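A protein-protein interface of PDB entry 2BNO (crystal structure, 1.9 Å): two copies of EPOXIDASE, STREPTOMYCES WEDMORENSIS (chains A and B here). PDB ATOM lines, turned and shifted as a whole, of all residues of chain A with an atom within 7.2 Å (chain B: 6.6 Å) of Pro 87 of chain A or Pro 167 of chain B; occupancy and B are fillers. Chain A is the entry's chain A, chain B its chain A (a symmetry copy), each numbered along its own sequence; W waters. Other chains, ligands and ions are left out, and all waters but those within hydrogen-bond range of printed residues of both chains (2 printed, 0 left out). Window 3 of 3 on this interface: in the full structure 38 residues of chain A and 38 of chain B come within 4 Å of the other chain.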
ATOM      1  N   GLN A  85      -3.620  22.726   2.853  1.00  0.00           N
ATOM      2  CA  GLN A  85      -2.333  23.375   2.853  1.00  0.00           C
ATOM      3  C   GLN A  85      -1.303  22.461   3.529  1.00  0.00           C
ATOM      4  O   GLN A  85      -1.509  22.008   4.667  1.00  0.00           O
ATOM      5  CB  GLN A  85      -2.412  24.721   3.560  1.00  0.00           C
ATOM      6  CG  GLN A  85      -1.109  25.496   3.486  1.00  0.00           C
ATOM      7  CD  GLN A  85      -0.954  26.459   4.621  1.00  0.00           C
ATOM      8  OE1 GLN A  85      -0.862  26.057   5.789  1.00  0.00           O
ATOM      9  NE2 GLN A  85      -0.939  27.731   4.302  1.00  0.00           N
ATOM     10  N   MET A  86      -0.189  22.203   2.831  1.00  0.00           N
ATOM     11  CA  MET A  86       0.874  21.328   3.344  1.00  0.00           C
ATOM     12  C   MET A  86       1.786  22.155   4.236  1.00  0.00           C
ATOM     13  O   MET A  86       1.900  23.356   4.020  1.00  0.00           O
ATOM     14  CB  MET A  86       1.633  20.682   2.169  1.00  0.00           C
ATOM     15  CG  MET A  86       0.730  19.799   1.257  1.00  0.00           C
ATOM     16  SD  MET A  86       0.157  18.256   2.024  1.00  0.00           S
ATOM     17  CE  MET A  86       1.677  17.325   2.049  1.00  0.00           C
ATOM     18  N   PRO A  87       2.421  21.555   5.250  1.00  0.00           N
ATOM     19  CA  PRO A  87       3.227  22.317   6.184  1.00  0.00           C
ATOM     20  C   PRO A  87       4.329  23.172   5.538  1.00  0.00           C
ATOM     21  O   PRO A  87       4.632  24.261   6.039  1.00  0.00           O
ATOM     22  CB  PRO A  87       3.823  21.239   7.111  1.00  0.00           C
ATOM     23  CG  PRO A  87       3.568  19.961   6.466  1.00  0.00           C
ATOM     24  CD  PRO A  87       2.351  20.130   5.628  1.00  0.00           C
ATOM     25  N   ASP A  88       4.889  22.714   4.422  1.00  0.00           N
ATOM     26  CA  ASP A  88       5.928  23.486   3.706  1.00  0.00           C
ATOM     27  C   ASP A  88       5.441  24.790   3.057  1.00  0.00           C
ATOM     28  O   ASP A  88       6.261  25.636   2.681  1.00  0.00           O
ATOM     29  CB  ASP A  88       6.565  22.622   2.614  1.00  0.00           C
ATOM     30  CG  ASP A  88       7.404  21.501   3.173  1.00  0.00           C
ATOM     31  OD1 ASP A  88       7.653  21.488   4.402  1.00  0.00           O
ATOM     32  OD2 ASP A  88       7.861  20.587   2.448  1.00  0.00           O
ATOM     33  N   GLU A  89       4.122  24.944   2.919  1.00  0.00           N
ATOM     34  CA  GLU A  89       3.519  26.019   2.117  1.00  0.00           C
ATOM     35  C   GLU A  89       2.985  27.213   2.906  1.00  0.00           C
ATOM     36  O   GLU A  89       2.194  28.002   2.379  1.00  0.00           O
ATOM     37  CB  GLU A  89       2.376  25.454   1.271  1.00  0.00           C
ATOM     38  CG  GLU A  89       2.799  24.949  -0.093  1.00  0.00           C
ATOM     39  CD  GLU A  89       3.265  23.513  -0.060  1.00  0.00           C
ATOM     40  OE1 GLU A  89       2.529  22.656  -0.592  1.00  0.00           O
ATOM     41  OE2 GLU A  89       4.353  23.239   0.499  1.00  0.00           O
ATOM     42  N   ARG A  90       3.395  27.348   4.160  1.00  0.00           N
ATOM     43  CA  ARG A  90       2.867  28.422   5.003  1.00  0.00           C
ATOM     44  C   ARG A  90       3.582  29.748   4.747  1.00  0.00           C
ATOM     45  O   ARG A  90       4.821  29.799   4.771  1.00  0.00           O
ATOM     46  CB  ARG A  90       3.008  28.081   6.488  1.00  0.00           C
ATOM     47  CG  ARG A  90       2.269  26.859   6.976  1.00  0.00           C
ATOM     48  CD  ARG A  90       2.620  26.568   8.403  1.00  0.00           C
ATOM     49  NE  ARG A  90       2.155  25.274   8.874  1.00  0.00           N
ATOM     50  CZ  ARG A  90       2.317  24.842  10.112  1.00  0.00           C
ATOM     51  NH1 ARG A  90       2.950  25.603  11.002  1.00  0.00           N
ATOM     52  NH2 ARG A  90       1.847  23.655  10.462  1.00  0.00           N
ATOM     53  N   PRO A  91       2.813  30.810   4.497  1.00  0.00           N
ATOM     54  CA  PRO A  91       3.334  32.186   4.560  1.00  0.00           C
ATOM     55  C   PRO A  91       3.565  32.648   6.012  1.00  0.00           C
ATOM     56  O   PRO A  91       2.773  32.309   6.909  1.00  0.00           O
ATOM     57  CB  PRO A  91       2.220  33.017   3.926  1.00  0.00           C
ATOM     58  CG  PRO A  91       1.311  32.020   3.282  1.00  0.00           C
ATOM     59  CD  PRO A  91       1.399  30.770   4.098  1.00  0.00           C
ATOM     60  N   ASN A 106       2.561  31.952  11.425  1.00  0.00           N
ATOM     61  CA  ASN A 106       2.586  30.968  10.385  1.00  0.00           C
ATOM     62  C   ASN A 106       1.144  30.788   9.860  1.00  0.00           C
ATOM     63  O   ASN A 106       0.283  30.207  10.554  1.00  0.00           O
ATOM     64  CB  ASN A 106       3.082  29.637  10.931  1.00  0.00           C
ATOM     65  CG  ASN A 106       4.058  28.956  10.005  1.00  0.00           C
ATOM     66  OD1 ASN A 106       4.789  27.971  10.532  1.00  0.00           O
ATOM     67  ND2 ASN A 106       4.171  29.313   8.827  1.00  0.00           N
ATOM     68  N   CYS A 107       0.880  31.279   8.651  1.00  0.00           N
ATOM     69  CA  CYS A 107      -0.500  31.279   8.111  1.00  0.00           C
ATOM     70  C   CYS A 107      -0.931  29.890   7.658  1.00  0.00           C
ATOM     71  O   CYS A 107      -0.263  29.261   6.817  1.00  0.00           O
ATOM     72  CB  CYS A 107      -0.671  32.376   7.002  1.00  0.00           C
ATOM     73  SG  CYS A 107      -0.598  34.090   7.667  1.00  0.00           S
ATOM     74  N   LEU A 108      -2.043  29.376   8.229  1.00  0.00           N
ATOM     75  CA  LEU A 108      -2.613  28.125   7.777  1.00  0.00           C
ATOM     76  C   LEU A 108      -3.623  28.344   6.628  1.00  0.00           C
ATOM     77  O   LEU A 108      -3.752  29.475   6.125  1.00  0.00           O
ATOM     78  CB  LEU A 108      -3.271  27.347   8.958  1.00  0.00           C
ATOM     79  CG  LEU A 108      -2.280  27.232  10.137  1.00  0.00           C
ATOM     80  CD1 LEU A 108      -3.001  26.642  11.367  1.00  0.00           C
ATOM     81  CD2 LEU A 108      -1.117  26.318   9.736  1.00  0.00           C
ATOM     82  N   VAL B 146      -3.441  18.832  11.466  1.00  0.00           N
ATOM     83  CA  VAL B 146      -2.905  17.520  11.815  1.00  0.00           C
ATOM     84  C   VAL B 146      -1.885  17.758  12.921  1.00  0.00           C
ATOM     85  O   VAL B 146      -0.855  18.374  12.694  1.00  0.00           O
ATOM     86  CB  VAL B 146      -2.229  16.807  10.615  1.00  0.00           C
ATOM     87  CG1 VAL B 146      -1.663  15.452  11.076  1.00  0.00           C
ATOM     88  CG2 VAL B 146      -3.237  16.596   9.486  1.00  0.00           C
ATOM     89  N   LEU B 147      -2.217  17.269  14.117  1.00  0.00           N
ATOM     90  CA  LEU B 147      -1.409  17.437  15.333  1.00  0.00           C
ATOM     91  C   LEU B 147      -0.285  16.408  15.440  1.00  0.00           C
ATOM     92  O   LEU B 147       0.856  16.746  15.787  1.00  0.00           O
ATOM     93  CB  LEU B 147      -2.303  17.222  16.543  1.00  0.00           C
ATOM     94  CG  LEU B 147      -3.136  18.348  17.076  1.00  0.00           C
ATOM     95  CD1 LEU B 147      -3.755  17.897  18.402  1.00  0.00           C
ATOM     96  CD2 LEU B 147      -2.261  19.576  17.238  1.00  0.00           C
ATOM     97  N   GLU B 148      -0.605  15.151  15.180  1.00  0.00           N
ATOM     98  CA  GLU B 148       0.426  14.092  15.287  1.00  0.00           C
ATOM     99  C   GLU B 148       0.220  13.090  14.189  1.00  0.00           C
ATOM    100  O   GLU B 148      -0.914  12.838  13.775  1.00  0.00           O
ATOM    101  CB  GLU B 148       0.339  13.363  16.643  1.00  0.00           C
ATOM    102  CG  GLU B 148       0.683  14.213  17.845  1.00  0.00           C
ATOM    103  CD  GLU B 148       0.457  13.481  19.174  1.00  0.00           C
ATOM    104  OE1 GLU B 148       0.195  12.238  19.143  1.00  0.00           O
ATOM    105  OE2 GLU B 148       0.518  14.162  20.228  1.00  0.00           O
ATOM    106  N   GLY B 149       1.313  12.514  13.709  1.00  0.00           N
ATOM    107  CA  GLY B 149       1.235  11.441  12.716  1.00  0.00           C
ATOM    108  C   GLY B 149       0.905  11.962  11.337  1.00  0.00           C
ATOM    109  O   GLY B 149       1.193  13.114  11.007  1.00  0.00           O
ATOM    110  N   GLU B 150       0.263  11.111  10.554  1.00  0.00           N
ATOM    111  CA  GLU B 150      -0.011  11.369   9.151  1.00  0.00           C
ATOM    112  C   GLU B 150      -1.391  10.815   8.869  1.00  0.00           C
ATOM    113  O   GLU B 150      -1.703   9.675   9.208  1.00  0.00           O
ATOM    114  CB  GLU B 150       1.071  10.707   8.255  1.00  0.00           C
ATOM    115  CG  GLU B 150       0.868  10.932   6.754  1.00  0.00           C
ATOM    116  CD  GLU B 150       1.855  10.124   5.900  1.00  0.00           C
ATOM    117  OE1 GLU B 150       2.642   9.292   6.451  1.00  0.00           O
ATOM    118  OE2 GLU B 150       1.845  10.344   4.678  1.00  0.00           O
ATOM    119  N   ILE B 151      -2.237  11.660   8.285  1.00  0.00           N
ATOM    120  CA  ILE B 151      -3.626  11.342   8.044  1.00  0.00           C
ATOM    121  C   ILE B 151      -3.835  11.037   6.571  1.00  0.00           C
ATOM    122  O   ILE B 151      -3.273  11.719   5.709  1.00  0.00           O
ATOM    123  CB  ILE B 151      -4.487  12.597   8.413  1.00  0.00           C
ATOM    124  CG1 ILE B 151      -4.457  12.794   9.943  1.00  0.00           C
ATOM    125  CG2 ILE B 151      -5.921  12.496   7.823  1.00  0.00           C
ATOM    126  CD1 ILE B 151      -5.420  11.850  10.679  1.00  0.00           C
ATOM    127  N   LEU B 165      -2.802  12.684   1.425  1.00  0.00           N
ATOM    128  CA  LEU B 165      -1.961  12.307   2.532  1.00  0.00           C
ATOM    129  C   LEU B 165      -1.405  13.577   3.187  1.00  0.00           C
ATOM    130  O   LEU B 165      -0.718  14.399   2.545  1.00  0.00           O
ATOM    131  CB  LEU B 165      -0.843  11.341   2.076  1.00  0.00           C
ATOM    132  CG  LEU B 165      -1.191   9.847   1.991  1.00  0.00           C
ATOM    133  CD1 LEU B 165      -1.407   9.199   3.366  1.00  0.00           C
ATOM    134  CD2 LEU B 165      -2.423   9.608   1.162  1.00  0.00           C
ATOM    135  N   LEU B 166      -1.727  13.740   4.467  1.00  0.00           N
ATOM    136  CA  LEU B 166      -1.538  14.987   5.197  1.00  0.00           C
ATOM    137  C   LEU B 166      -0.616  14.783   6.388  1.00  0.00           C
ATOM    138  O   LEU B 166      -1.053  14.234   7.399  1.00  0.00           O
ATOM    139  CB  LEU B 166      -2.898  15.464   5.718  1.00  0.00           C
ATOM    140  CG  LEU B 166      -3.920  15.692   4.603  1.00  0.00           C
ATOM    141  CD1 LEU B 166      -5.309  15.827   5.211  1.00  0.00           C
ATOM    142  CD2 LEU B 166      -3.519  16.939   3.802  1.00  0.00           C
ATOM    143  N   PRO B 167       0.643  15.197   6.264  1.00  0.00           N
ATOM    144  CA  PRO B 167       1.610  15.063   7.348  1.00  0.00           C
ATOM    145  C   PRO B 167       1.316  16.016   8.481  1.00  0.00           C
ATOM    146  O   PRO B 167       0.446  16.911   8.350  1.00  0.00           O
ATOM    147  CB  PRO B 167       2.930  15.444   6.681  1.00  0.00           C
ATOM    148  CG  PRO B 167       2.555  16.367   5.613  1.00  0.00           C
ATOM    149  CD  PRO B 167       1.269  15.757   5.045  1.00  0.00           C
ATOM    150  N   THR B 168       2.023  15.816   9.588  1.00  0.00           N
ATOM    151  CA  THR B 168       1.873  16.668  10.752  1.00  0.00           C
ATOM    152  C   THR B 168       2.023  18.133  10.358  1.00  0.00           C
ATOM    153  O   THR B 168       2.942  18.503   9.638  1.00  0.00           O
ATOM    154  CB  THR B 168       2.919  16.258  11.837  1.00  0.00           C
ATOM    155  OG1 THR B 168       2.549  14.982  12.326  1.00  0.00           O
ATOM    156  CG2 THR B 168       2.806  17.110  13.062  1.00  0.00           C
ATOM    157  N   GLY B 169       1.101  18.969  10.833  1.00  0.00           N
ATOM    158  CA  GLY B 169       1.198  20.382  10.556  1.00  0.00           C
ATOM    159  C   GLY B 169       0.372  20.773   9.318  1.00  0.00           C
ATOM    160  O   GLY B 169       0.202  21.964   9.069  1.00  0.00           O
ATOM    161  N   ALA B 170      -0.137  19.795   8.552  1.00  0.00           N
ATOM    162  CA  ALA B 170      -1.014  20.119   7.415  1.00  0.00           C
ATOM    163  C   ALA B 170      -2.330  20.741   7.942  1.00  0.00           C
ATOM    164  O   ALA B 170      -2.774  20.428   9.067  1.00  0.00           O
ATOM    165  CB  ALA B 170      -1.312  18.871   6.561  1.00  0.00           C
ATOM    166  N   SER B 171      -2.955  21.599   7.142  1.00  0.00           N
ATOM    167  CA  SER B 171      -4.275  22.115   7.543  1.00  0.00           C
ATOM    168  C   SER B 171      -5.275  21.961   6.391  1.00  0.00           C
ATOM    169  O   SER B 171      -4.875  21.842   5.221  1.00  0.00           O
ATOM    170  CB  SER B 171      -4.172  23.542   8.055  1.00  0.00           C
ATOM    171  OG  SER B 171      -3.642  24.383   7.046  1.00  0.00           O
HETATM  172  O   HOH W   1      -0.590  23.992   7.129  1.00  0.00           O
HETATM  173  O   HOH W   2      -1.525  15.819   0.191  1.00  0.00           O
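Printed residues of chain B within 4 Å of Gln 85 of chain A: Ala 170 and Ser 171. Of chain B, only Pro 167 (3.8 Å), Thr 168 (3.5 Å) and Ala 170 (3.8 Å) come within 4 Å of Pro 87 of chain A. Asp 88 of chain A touches none of the printed residues of chain B. Printed residues of chain B within 4 Å of Arg 90 of chain A: Gly 169 (2.7 Å). Ile 151 of chain B touches none of the printed residues of chain A. Of chain A, only Met 86 (3.4 Å) and Pro 87 (3.8 Å) come within 4 Å of Pro 167 of chain B. Printed residues of chain A within 4 Å of Ala 170 of chain B: Gln 85 (3.4 Å) and Pro 87 (3.8 Å). The nearest residue of chain A that does not touch Pro 167 of chain B is Gln 85 of chain A (6.6 Å). The nearest printed residue of chain A that does not touch Leu 165 of chain B is Pro 87 of chain A (7.2 Å).
Among the printed residues, merely in contact across the chains: Gln 85 of chain A with Ala 170 of chain B, Met 86 of chain A with Pro 167 of chain B, Leu 108 of chain A with Ser 171 of chain B, Pro 87 of chain A with Thr 168 of chain B, Pro 87 of chain A with Pro 167 of chain B, Pro 87 of chain A with Ala 170 of chain B and Met 86 of chain A with Leu 165 of chain B.
No position is printed for both chains.
O of Val 146 of chain B is in hydrogen-bond range of N of Gly 169 of chain B (2.8 Å). N of Val 146 of chain B lies within hydrogen-bond range of O of Ala 170 of chain B (3.0 Å). The side-chain hydroxyl (OG1) of Thr 168 of chain B sits at hydrogen-bond distance from the backbone carbonyl oxygen (O) of Gly 149 of chain B (2.7 Å). The guanidinium group (NH1) of Arg 90 of chain A is in hydrogen-bond range of the side-chain amide oxygen (OD1) of Asn 106 of chain A (3.0 Å). NE2 of Gln 85 of chain A is in hydrogen-bond range of O of Cys 107 of chain A, at 3.0 Å.
Of the 13 printed residues of chain B, 6 touch a printed residue of chain A. Hydrophobic or aromatic side chains of chain B within 4 Å of the printed part of chain A: Pro 167 and Ala 170. Of the 10 printed residues of chain A, 5 touch a printed residue of chain B. Printed residues of chain A that touch a printed residue of chain B: Gln 85, Met 86, Pro 87, Arg 90 and Leu 108. Hydrophobic or aromatic side chains of chain A within 4 Å of the printed part of chain B: Met 86, Pro 87 and Leu 108. Among the printed residues, no Asp or Glu carboxylate lies within 4 Å of a Lys or Arg side-chain nitrogen of the other chain.
The backbone NH of Gln 85 of chain A sits at hydrogen-bond distance from the backbone carbonyl oxygen of Ser 171 of chain B, 2.8 Å away. O of Gly 169 of chain B lies within hydrogen-bond range of NH2 of Arg 90 of chain A, at 2.7 Å.
Water W1 lies within hydrogen-bond range of OE1 of Gln 85 of chain A, O of Gly 169 of chain B, OG of Ser 171 of chain B and NE of Arg 90 of chain A. Water W2 lies within hydrogen-bond range of the backbone carbonyl oxygen (O) of Leu 165 of chain B (2.9 Å) and the side-chain sulfur (SD) of Met 86 of chain A (3.5 Å).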
